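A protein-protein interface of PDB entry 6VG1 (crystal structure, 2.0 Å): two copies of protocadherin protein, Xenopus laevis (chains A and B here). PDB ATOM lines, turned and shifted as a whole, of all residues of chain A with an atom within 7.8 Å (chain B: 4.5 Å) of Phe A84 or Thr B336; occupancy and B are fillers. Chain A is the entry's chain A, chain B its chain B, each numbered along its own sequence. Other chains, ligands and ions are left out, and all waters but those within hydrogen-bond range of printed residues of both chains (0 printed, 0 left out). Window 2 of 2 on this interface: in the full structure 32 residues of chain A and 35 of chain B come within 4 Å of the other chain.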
ATOM      1  N   SER A  31      23.170  -1.335  30.481  1.00  0.00           N
ATOM      2  CA  SER A  31      23.554  -2.590  29.846  1.00  0.00           C
ATOM      3  C   SER A  31      24.851  -2.331  29.085  1.00  0.00           C
ATOM      4  O   SER A  31      24.887  -2.420  27.853  1.00  0.00           O
ATOM      5  CB  SER A  31      22.443  -3.099  28.928  1.00  0.00           C
ATOM      6  OG  SER A  31      22.740  -4.404  28.456  1.00  0.00           O
ATOM      7  N   VAL A  77      28.056   1.561  24.826  1.00  0.00           N
ATOM      8  CA  VAL A  77      26.653   1.922  24.695  1.00  0.00           C
ATOM      9  C   VAL A  77      25.912   1.382  25.904  1.00  0.00           C
ATOM     10  O   VAL A  77      26.196   0.275  26.378  1.00  0.00           O
ATOM     11  CB  VAL A  77      26.047   1.387  23.381  1.00  0.00           C
ATOM     12  CG1 VAL A  77      26.686   2.078  22.192  1.00  0.00           C
ATOM     13  CG2 VAL A  77      26.213  -0.112  23.282  1.00  0.00           C
ATOM     14  N   SER A  78      24.964   2.168  26.403  1.00  0.00           N
ATOM     15  CA  SER A  78      24.164   1.808  27.560  1.00  0.00           C
ATOM     16  C   SER A  78      22.699   2.023  27.221  1.00  0.00           C
ATOM     17  O   SER A  78      22.349   2.538  26.158  1.00  0.00           O
ATOM     18  CB  SER A  78      24.555   2.629  28.797  1.00  0.00           C
ATOM     19  OG  SER A  78      24.626   4.011  28.493  1.00  0.00           O
ATOM     20  N   VAL A  79      21.841   1.599  28.139  1.00  0.00           N
ATOM     21  CA  VAL A  79      20.401   1.756  28.000  1.00  0.00           C
ATOM     22  C   VAL A  79      19.858   2.234  29.337  1.00  0.00           C
ATOM     23  O   VAL A  79      20.000   1.543  30.351  1.00  0.00           O
ATOM     24  CB  VAL A  79      19.714   0.449  27.570  1.00  0.00           C
ATOM     25  CG1 VAL A  79      20.202   0.034  26.191  1.00  0.00           C
ATOM     26  CG2 VAL A  79      19.989  -0.657  28.574  1.00  0.00           C
ATOM     27  N   ALA A  80      19.259   3.421  29.348  1.00  0.00           N
ATOM     28  CA  ALA A  80      18.690   4.007  30.556  1.00  0.00           C
ATOM     29  C   ALA A  80      17.269   4.448  30.236  1.00  0.00           C
ATOM     30  O   ALA A  80      17.069   5.435  29.521  1.00  0.00           O
ATOM     31  CB  ALA A  80      19.530   5.183  31.054  1.00  0.00           C
ATOM     32  N   LYS A  81      16.287   3.715  30.761  1.00  0.00           N
ATOM     33  CA  LYS A  81      14.873   4.013  30.531  1.00  0.00           C
ATOM     34  C   LYS A  81      14.507   3.864  29.052  1.00  0.00           C
ATOM     35  O   LYS A  81      13.823   4.711  28.474  1.00  0.00           O
ATOM     36  CB  LYS A  81      14.516   5.412  31.038  1.00  0.00           C
ATOM     37  CG  LYS A  81      14.557   5.602  32.553  1.00  0.00           C
ATOM     38  CD  LYS A  81      14.138   7.039  32.924  1.00  0.00           C
ATOM     39  CE  LYS A  81      14.203   7.312  34.421  1.00  0.00           C
ATOM     40  NZ  LYS A  81      13.839   8.731  34.741  1.00  0.00           N
ATOM     41  N   GLU A  82      14.977   2.780  28.438  1.00  0.00           N
ATOM     42  CA  GLU A  82      14.692   2.433  27.048  1.00  0.00           C
ATOM     43  C   GLU A  82      15.275   3.424  26.050  1.00  0.00           C
ATOM     44  O   GLU A  82      14.843   3.467  24.896  1.00  0.00           O
ATOM     45  CB  GLU A  82      13.186   2.301  26.813  1.00  0.00           C
ATOM     46  CG  GLU A  82      12.529   1.178  27.582  1.00  0.00           C
ATOM     47  CD  GLU A  82      13.057  -0.183  27.194  1.00  0.00           C
ATOM     48  OE1 GLU A  82      13.756  -0.289  26.165  1.00  0.00           O
ATOM     49  OE2 GLU A  82      12.749  -1.158  27.908  1.00  0.00           O
ATOM     50  N   GLN A  83      16.238   4.232  26.468  1.00  0.00           N
ATOM     51  CA  GLN A  83      17.004   5.081  25.564  1.00  0.00           C
ATOM     52  C   GLN A  83      18.401   4.491  25.433  1.00  0.00           C
ATOM     53  O   GLN A  83      19.120   4.379  26.431  1.00  0.00           O
ATOM     54  CB  GLN A  83      17.069   6.520  26.078  1.00  0.00           C
ATOM     55  CG  GLN A  83      18.312   7.284  25.650  1.00  0.00           C
ATOM     56  CD  GLN A  83      18.253   8.749  26.051  1.00  0.00           C
ATOM     57  OE1 GLN A  83      18.112   9.626  25.202  1.00  0.00           O
ATOM     58  NE2 GLN A  83      18.353   9.019  27.347  1.00  0.00           N
ATOM     59  N   PHE A  84      18.773   4.099  24.214  1.00  0.00           N
ATOM     60  CA  PHE A  84      20.136   3.661  23.943  1.00  0.00           C
ATOM     61  C   PHE A  84      21.060   4.871  23.900  1.00  0.00           C
ATOM     62  O   PHE A  84      20.806   5.828  23.162  1.00  0.00           O
ATOM     63  CB  PHE A  84      20.216   2.913  22.613  1.00  0.00           C
ATOM     64  CG  PHE A  84      19.274   1.760  22.508  1.00  0.00           C
ATOM     65  CD1 PHE A  84      19.649   0.501  22.941  1.00  0.00           C
ATOM     66  CD2 PHE A  84      18.018   1.932  21.958  1.00  0.00           C
ATOM     67  CE1 PHE A  84      18.785  -0.563  22.834  1.00  0.00           C
ATOM     68  CE2 PHE A  84      17.148   0.873  21.849  1.00  0.00           C
ATOM     69  CZ  PHE A  84      17.533  -0.380  22.286  1.00  0.00           C
ATOM     70  N   LYS A  85      22.141   4.822  24.670  1.00  0.00           N
ATOM     71  CA  LYS A  85      23.100   5.910  24.708  1.00  0.00           C
ATOM     72  C   LYS A  85      24.462   5.432  24.226  1.00  0.00           C
ATOM     73  O   LYS A  85      24.735   4.233  24.156  1.00  0.00           O
ATOM     74  CB  LYS A  85      23.262   6.478  26.115  1.00  0.00           C
ATOM     75  CG  LYS A  85      22.019   7.106  26.721  1.00  0.00           C
ATOM     76  CD  LYS A  85      22.417   7.990  27.899  1.00  0.00           C
ATOM     77  CE  LYS A  85      21.279   8.178  28.877  1.00  0.00           C
ATOM     78  NZ  LYS A  85      21.598   9.219  29.899  1.00  0.00           N
ATOM     79  N   LEU A  86      25.317   6.394  23.892  1.00  0.00           N
ATOM     80  CA  LEU A  86      26.693   6.118  23.512  1.00  0.00           C
ATOM     81  C   LEU A  86      27.609   7.051  24.284  1.00  0.00           C
ATOM     82  O   LEU A  86      27.352   8.257  24.368  1.00  0.00           O
ATOM     83  CB  LEU A  86      26.918   6.298  22.012  1.00  0.00           C
ATOM     84  CG  LEU A  86      28.346   6.029  21.538  1.00  0.00           C
ATOM     85  CD1 LEU A  86      28.267   5.483  20.109  1.00  0.00           C
ATOM     86  CD2 LEU A  86      29.228   7.239  21.587  1.00  0.00           C
ATOM     87  N   LEU B 325      24.542  -0.400  16.263  1.00  0.00           N
ATOM     88  CA  LEU B 325      24.391  -1.005  17.582  1.00  0.00           C
ATOM     89  C   LEU B 325      23.965  -2.463  17.465  1.00  0.00           C
ATOM     90  O   LEU B 325      24.466  -3.327  18.192  1.00  0.00           O
ATOM     91  CB  LEU B 325      23.367  -0.229  18.415  1.00  0.00           C
ATOM     92  CG  LEU B 325      22.859  -0.977  19.645  1.00  0.00           C
ATOM     93  CD1 LEU B 325      23.853  -0.807  20.800  1.00  0.00           C
ATOM     94  CD2 LEU B 325      21.468  -0.513  20.074  1.00  0.00           C
ATOM     95  N   ILE B 335      16.619  -1.646  15.176  1.00  0.00           N
ATOM     96  CA  ILE B 335      16.346  -1.006  16.453  1.00  0.00           C
ATOM     97  C   ILE B 335      14.904  -1.299  16.829  1.00  0.00           C
ATOM     98  O   ILE B 335      14.014  -1.321  15.974  1.00  0.00           O
ATOM     99  CB  ILE B 335      16.641   0.511  16.403  1.00  0.00           C
ATOM    100  CG1 ILE B 335      16.433   1.112  17.788  1.00  0.00           C
ATOM    101  CG2 ILE B 335      15.781   1.186  15.365  1.00  0.00           C
ATOM    102  CD1 ILE B 335      16.894   2.539  17.899  1.00  0.00           C
ATOM    103  N   THR B 336      14.686  -1.544  18.119  1.00  0.00           N
ATOM    104  CA  THR B 336      13.363  -1.893  18.613  1.00  0.00           C
ATOM    105  C   THR B 336      12.435  -0.686  18.547  1.00  0.00           C
ATOM    106  O   THR B 336      12.832   0.440  18.864  1.00  0.00           O
ATOM    107  CB  THR B 336      13.448  -2.392  20.056  1.00  0.00           C
ATOM    108  OG1 THR B 336      12.168  -2.887  20.465  1.00  0.00           O
ATOM    109  CG2 THR B 336      13.867  -1.259  20.990  1.00  0.00           C
ATOM    110  N   GLU B 337      11.178  -0.927  18.165  1.00  0.00           N
ATOM    111  CA  GLU B 337      10.193   0.149  18.172  1.00  0.00           C
ATOM    112  C   GLU B 337      10.025   0.760  19.560  1.00  0.00           C
ATOM    113  O   GLU B 337       9.447   1.847  19.679  1.00  0.00           O
ATOM    114  CB  GLU B 337       8.842  -0.356  17.631  1.00  0.00           C
ATOM    115  CG  GLU B 337       8.239  -1.592  18.312  1.00  0.00           C
ATOM    116  CD  GLU B 337       6.889  -1.998  17.720  1.00  0.00           C
ATOM    117  OE1 GLU B 337       6.068  -1.109  17.403  1.00  0.00           O
ATOM    118  OE2 GLU B 337       6.637  -3.214  17.586  1.00  0.00           O
ATOM    119  N   ALA B 338      10.541   0.102  20.601  1.00  0.00           N
ATOM    120  CA  ALA B 338      10.436   0.583  21.972  1.00  0.00           C
ATOM    121  C   ALA B 338      11.409   1.708  22.300  1.00  0.00           C
ATOM    122  O   ALA B 338      11.259   2.341  23.348  1.00  0.00           O
ATOM    123  CB  ALA B 338      10.669  -0.578  22.946  1.00  0.00           C
ATOM    124  N   ALA B 339      12.394   1.973  21.445  1.00  0.00           N
ATOM    125  CA  ALA B 339      13.417   2.954  21.780  1.00  0.00           C
ATOM    126  C   ALA B 339      12.783   4.310  22.050  1.00  0.00           C
ATOM    127  O   ALA B 339      11.809   4.701  21.401  1.00  0.00           O
ATOM    128  CB  ALA B 339      14.434   3.075  20.649  1.00  0.00           C
ATOM    129  N   GLU B 342      15.748  10.120  20.873  1.00  0.00           N
ATOM    130  CA  GLU B 342      17.188  10.362  20.944  1.00  0.00           C
ATOM    131  C   GLU B 342      17.938   9.121  21.427  1.00  0.00           C
ATOM    132  O   GLU B 342      18.813   9.185  22.292  1.00  0.00           O
ATOM    133  CB  GLU B 342      17.479  11.575  21.830  1.00  0.00           C
ATOM    134  CG  GLU B 342      16.857  12.860  21.294  1.00  0.00           C
ATOM    135  CD  GLU B 342      17.191  14.086  22.127  1.00  0.00           C
ATOM    136  OE1 GLU B 342      18.122  14.012  22.958  1.00  0.00           O
ATOM    137  OE2 GLU B 342      16.511  15.123  21.952  1.00  0.00           O
ATOM    138  N   SER B 343      17.590   7.981  20.845  1.00  0.00           N
ATOM    139  CA  SER B 343      18.324   6.744  21.063  1.00  0.00           C
ATOM    140  C   SER B 343      19.348   6.558  19.950  1.00  0.00           C
ATOM    141  O   SER B 343      19.085   6.872  18.785  1.00  0.00           O
ATOM    142  CB  SER B 343      17.366   5.554  21.110  1.00  0.00           C
ATOM    143  OG  SER B 343      16.466   5.692  22.192  1.00  0.00           O
ATOM    144  N   PHE B 344      20.520   6.050  20.319  1.00  0.00           N
ATOM    145  CA  PHE B 344      21.585   5.813  19.355  1.00  0.00           C
ATOM    146  C   PHE B 344      21.255   4.589  18.508  1.00  0.00           C
ATOM    147  O   PHE B 344      20.955   3.517  19.044  1.00  0.00           O
ATOM    148  CB  PHE B 344      22.920   5.618  20.077  1.00  0.00           C
ATOM    149  CG  PHE B 344      23.964   4.941  19.239  1.00  0.00           C
ATOM    150  CD1 PHE B 344      24.812   5.675  18.430  1.00  0.00           C
ATOM    151  CD2 PHE B 344      24.099   3.563  19.264  1.00  0.00           C
ATOM    152  CE1 PHE B 344      25.770   5.044  17.653  1.00  0.00           C
ATOM    153  CE2 PHE B 344      25.052   2.931  18.494  1.00  0.00           C
ATOM    154  CZ  PHE B 344      25.890   3.676  17.684  1.00  0.00           C
ATOM    155  N   VAL B 421      13.054  -1.493  11.826  1.00  0.00           N
ATOM    156  CA  VAL B 421      12.495  -1.388  13.166  1.00  0.00           C
ATOM    157  C   VAL B 421      12.069  -2.775  13.625  1.00  0.00           C
ATOM    158  O   VAL B 421      11.331  -3.473  12.919  1.00  0.00           O
ATOM    159  CB  VAL B 421      11.316  -0.404  13.188  1.00  0.00           C
ATOM    160  CG1 VAL B 421      10.803  -0.225  14.599  1.00  0.00           C
ATOM    161  CG2 VAL B 421      11.745   0.935  12.606  1.00  0.00           C
ATOM    162  N   SER B 422      12.528  -3.168  14.811  1.00  0.00           N
ATOM    163  CA  SER B 422      12.261  -4.492  15.353  1.00  0.00           C
ATOM    164  C   SER B 422      10.927  -4.517  16.080  1.00  0.00           C
ATOM    165  O   SER B 422      10.582  -3.571  16.793  1.00  0.00           O
ATOM    166  CB  SER B 422      13.373  -4.910  16.314  1.00  0.00           C
ATOM    167  OG  SER B 422      13.233  -6.276  16.669  1.00  0.00           O
ATOM    168  N   GLU B 424       8.032  -5.179  18.669  1.00  0.00           N
ATOM    169  CA  GLU B 424       7.687  -5.459  20.051  1.00  0.00           C
ATOM    170  C   GLU B 424       6.186  -5.713  20.100  1.00  0.00           C
ATOM    171  O   GLU B 424       5.442  -5.346  19.186  1.00  0.00           O
ATOM    172  CB  GLU B 424       8.082  -4.311  20.982  1.00  0.00           C
ATOM    173  CG  GLU B 424       9.574  -4.009  20.989  1.00  0.00           C
ATOM    174  CD  GLU B 424      10.424  -5.173  21.478  1.00  0.00           C
ATOM    175  OE1 GLU B 424       9.952  -5.935  22.349  1.00  0.00           O
ATOM    176  OE2 GLU B 424      11.565  -5.327  20.986  1.00  0.00           O
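The side-chain amide oxygen (OE1) of Gln A83 sits close to the backbone carbonyl oxygen (O) of Glu B342 (3.0 Å). The backbone NH (N) of Phe A84 sits at hydrogen-bond distance from the side-chain hydroxyl (OG) of Ser B343, at 3.5 Å. The backbone carbonyl oxygen of Phe A84 is in hydrogen-bond range of the backbone NH of Phe B344, 2.9 Å away.
The side-chain hydroxyl (OG1) of Thr B336 lies close to the backbone NH (N) of Ala B338 (3.4 Å). OG1 of Thr B336 is in hydrogen-bond range of OE2 of Glu B424 (2.6 Å).
CG2 of Val A77 touches CD1 of Leu B325, 3.5 Å away. Glu A82 touches Ala B338 (CB to O, 3.96 Å). O of Glu A82 touches CA of Ala B339, 3.5 Å away. OG of Ser B343 touches O of Glu A82, 3.9 Å away. Gln A83 touches Ser B343. Phe A84 touches Leu B325. CZ of Phe A84 touches CG2 of Thr B336, at 3.99 Å. CE2 of Phe A84 touches CB of Ala B339, 3.7 Å away. O of Glu B342 touches O of Phe A84, at 3.9998 Å. CD1 of Leu A86 touches CE1 of Phe B344 (3.5 Å).
Of the printed residues of chain B, Glu A82 touches Ala B338, Ala B339 and Ser B343. Printed residues of chain B within 4 Å of Phe A84: Leu B325, Thr B336, Ala B339, Glu B342, Ser B343 and Phe B344. Of the printed residues of chain B, Leu A86 touches Phe B344. Of the printed residues of chain A, Leu B325 touches Val A77 (3.5 Å) and Phe A84 (3.5 Å). Printed residues of chain A within 4 Å of Thr B336: Phe A84. Glu B337 touches none of the printed residues of chain A. Printed residues of chain A within 4 Å of Ala B339: Glu A82 (3.5 Å) and Phe A84 (3.7 Å). Ser B422 touches none of the printed residues of chain A. The nearest printed residue of chain B that does not touch Gln A83 is Ala B339 (5.5 Å).
Hydrophobic or aromatic side chains of chain A within 4 Å of the printed part of chain B: Val A77, Phe A84 and Leu A86. Among the printed residues, 13 pairs touch across the chains.
No position is printed for both chains. Of the 13 pairs that touch across the chains among the printed residues, none has its exchanged pair printed and touching as well.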
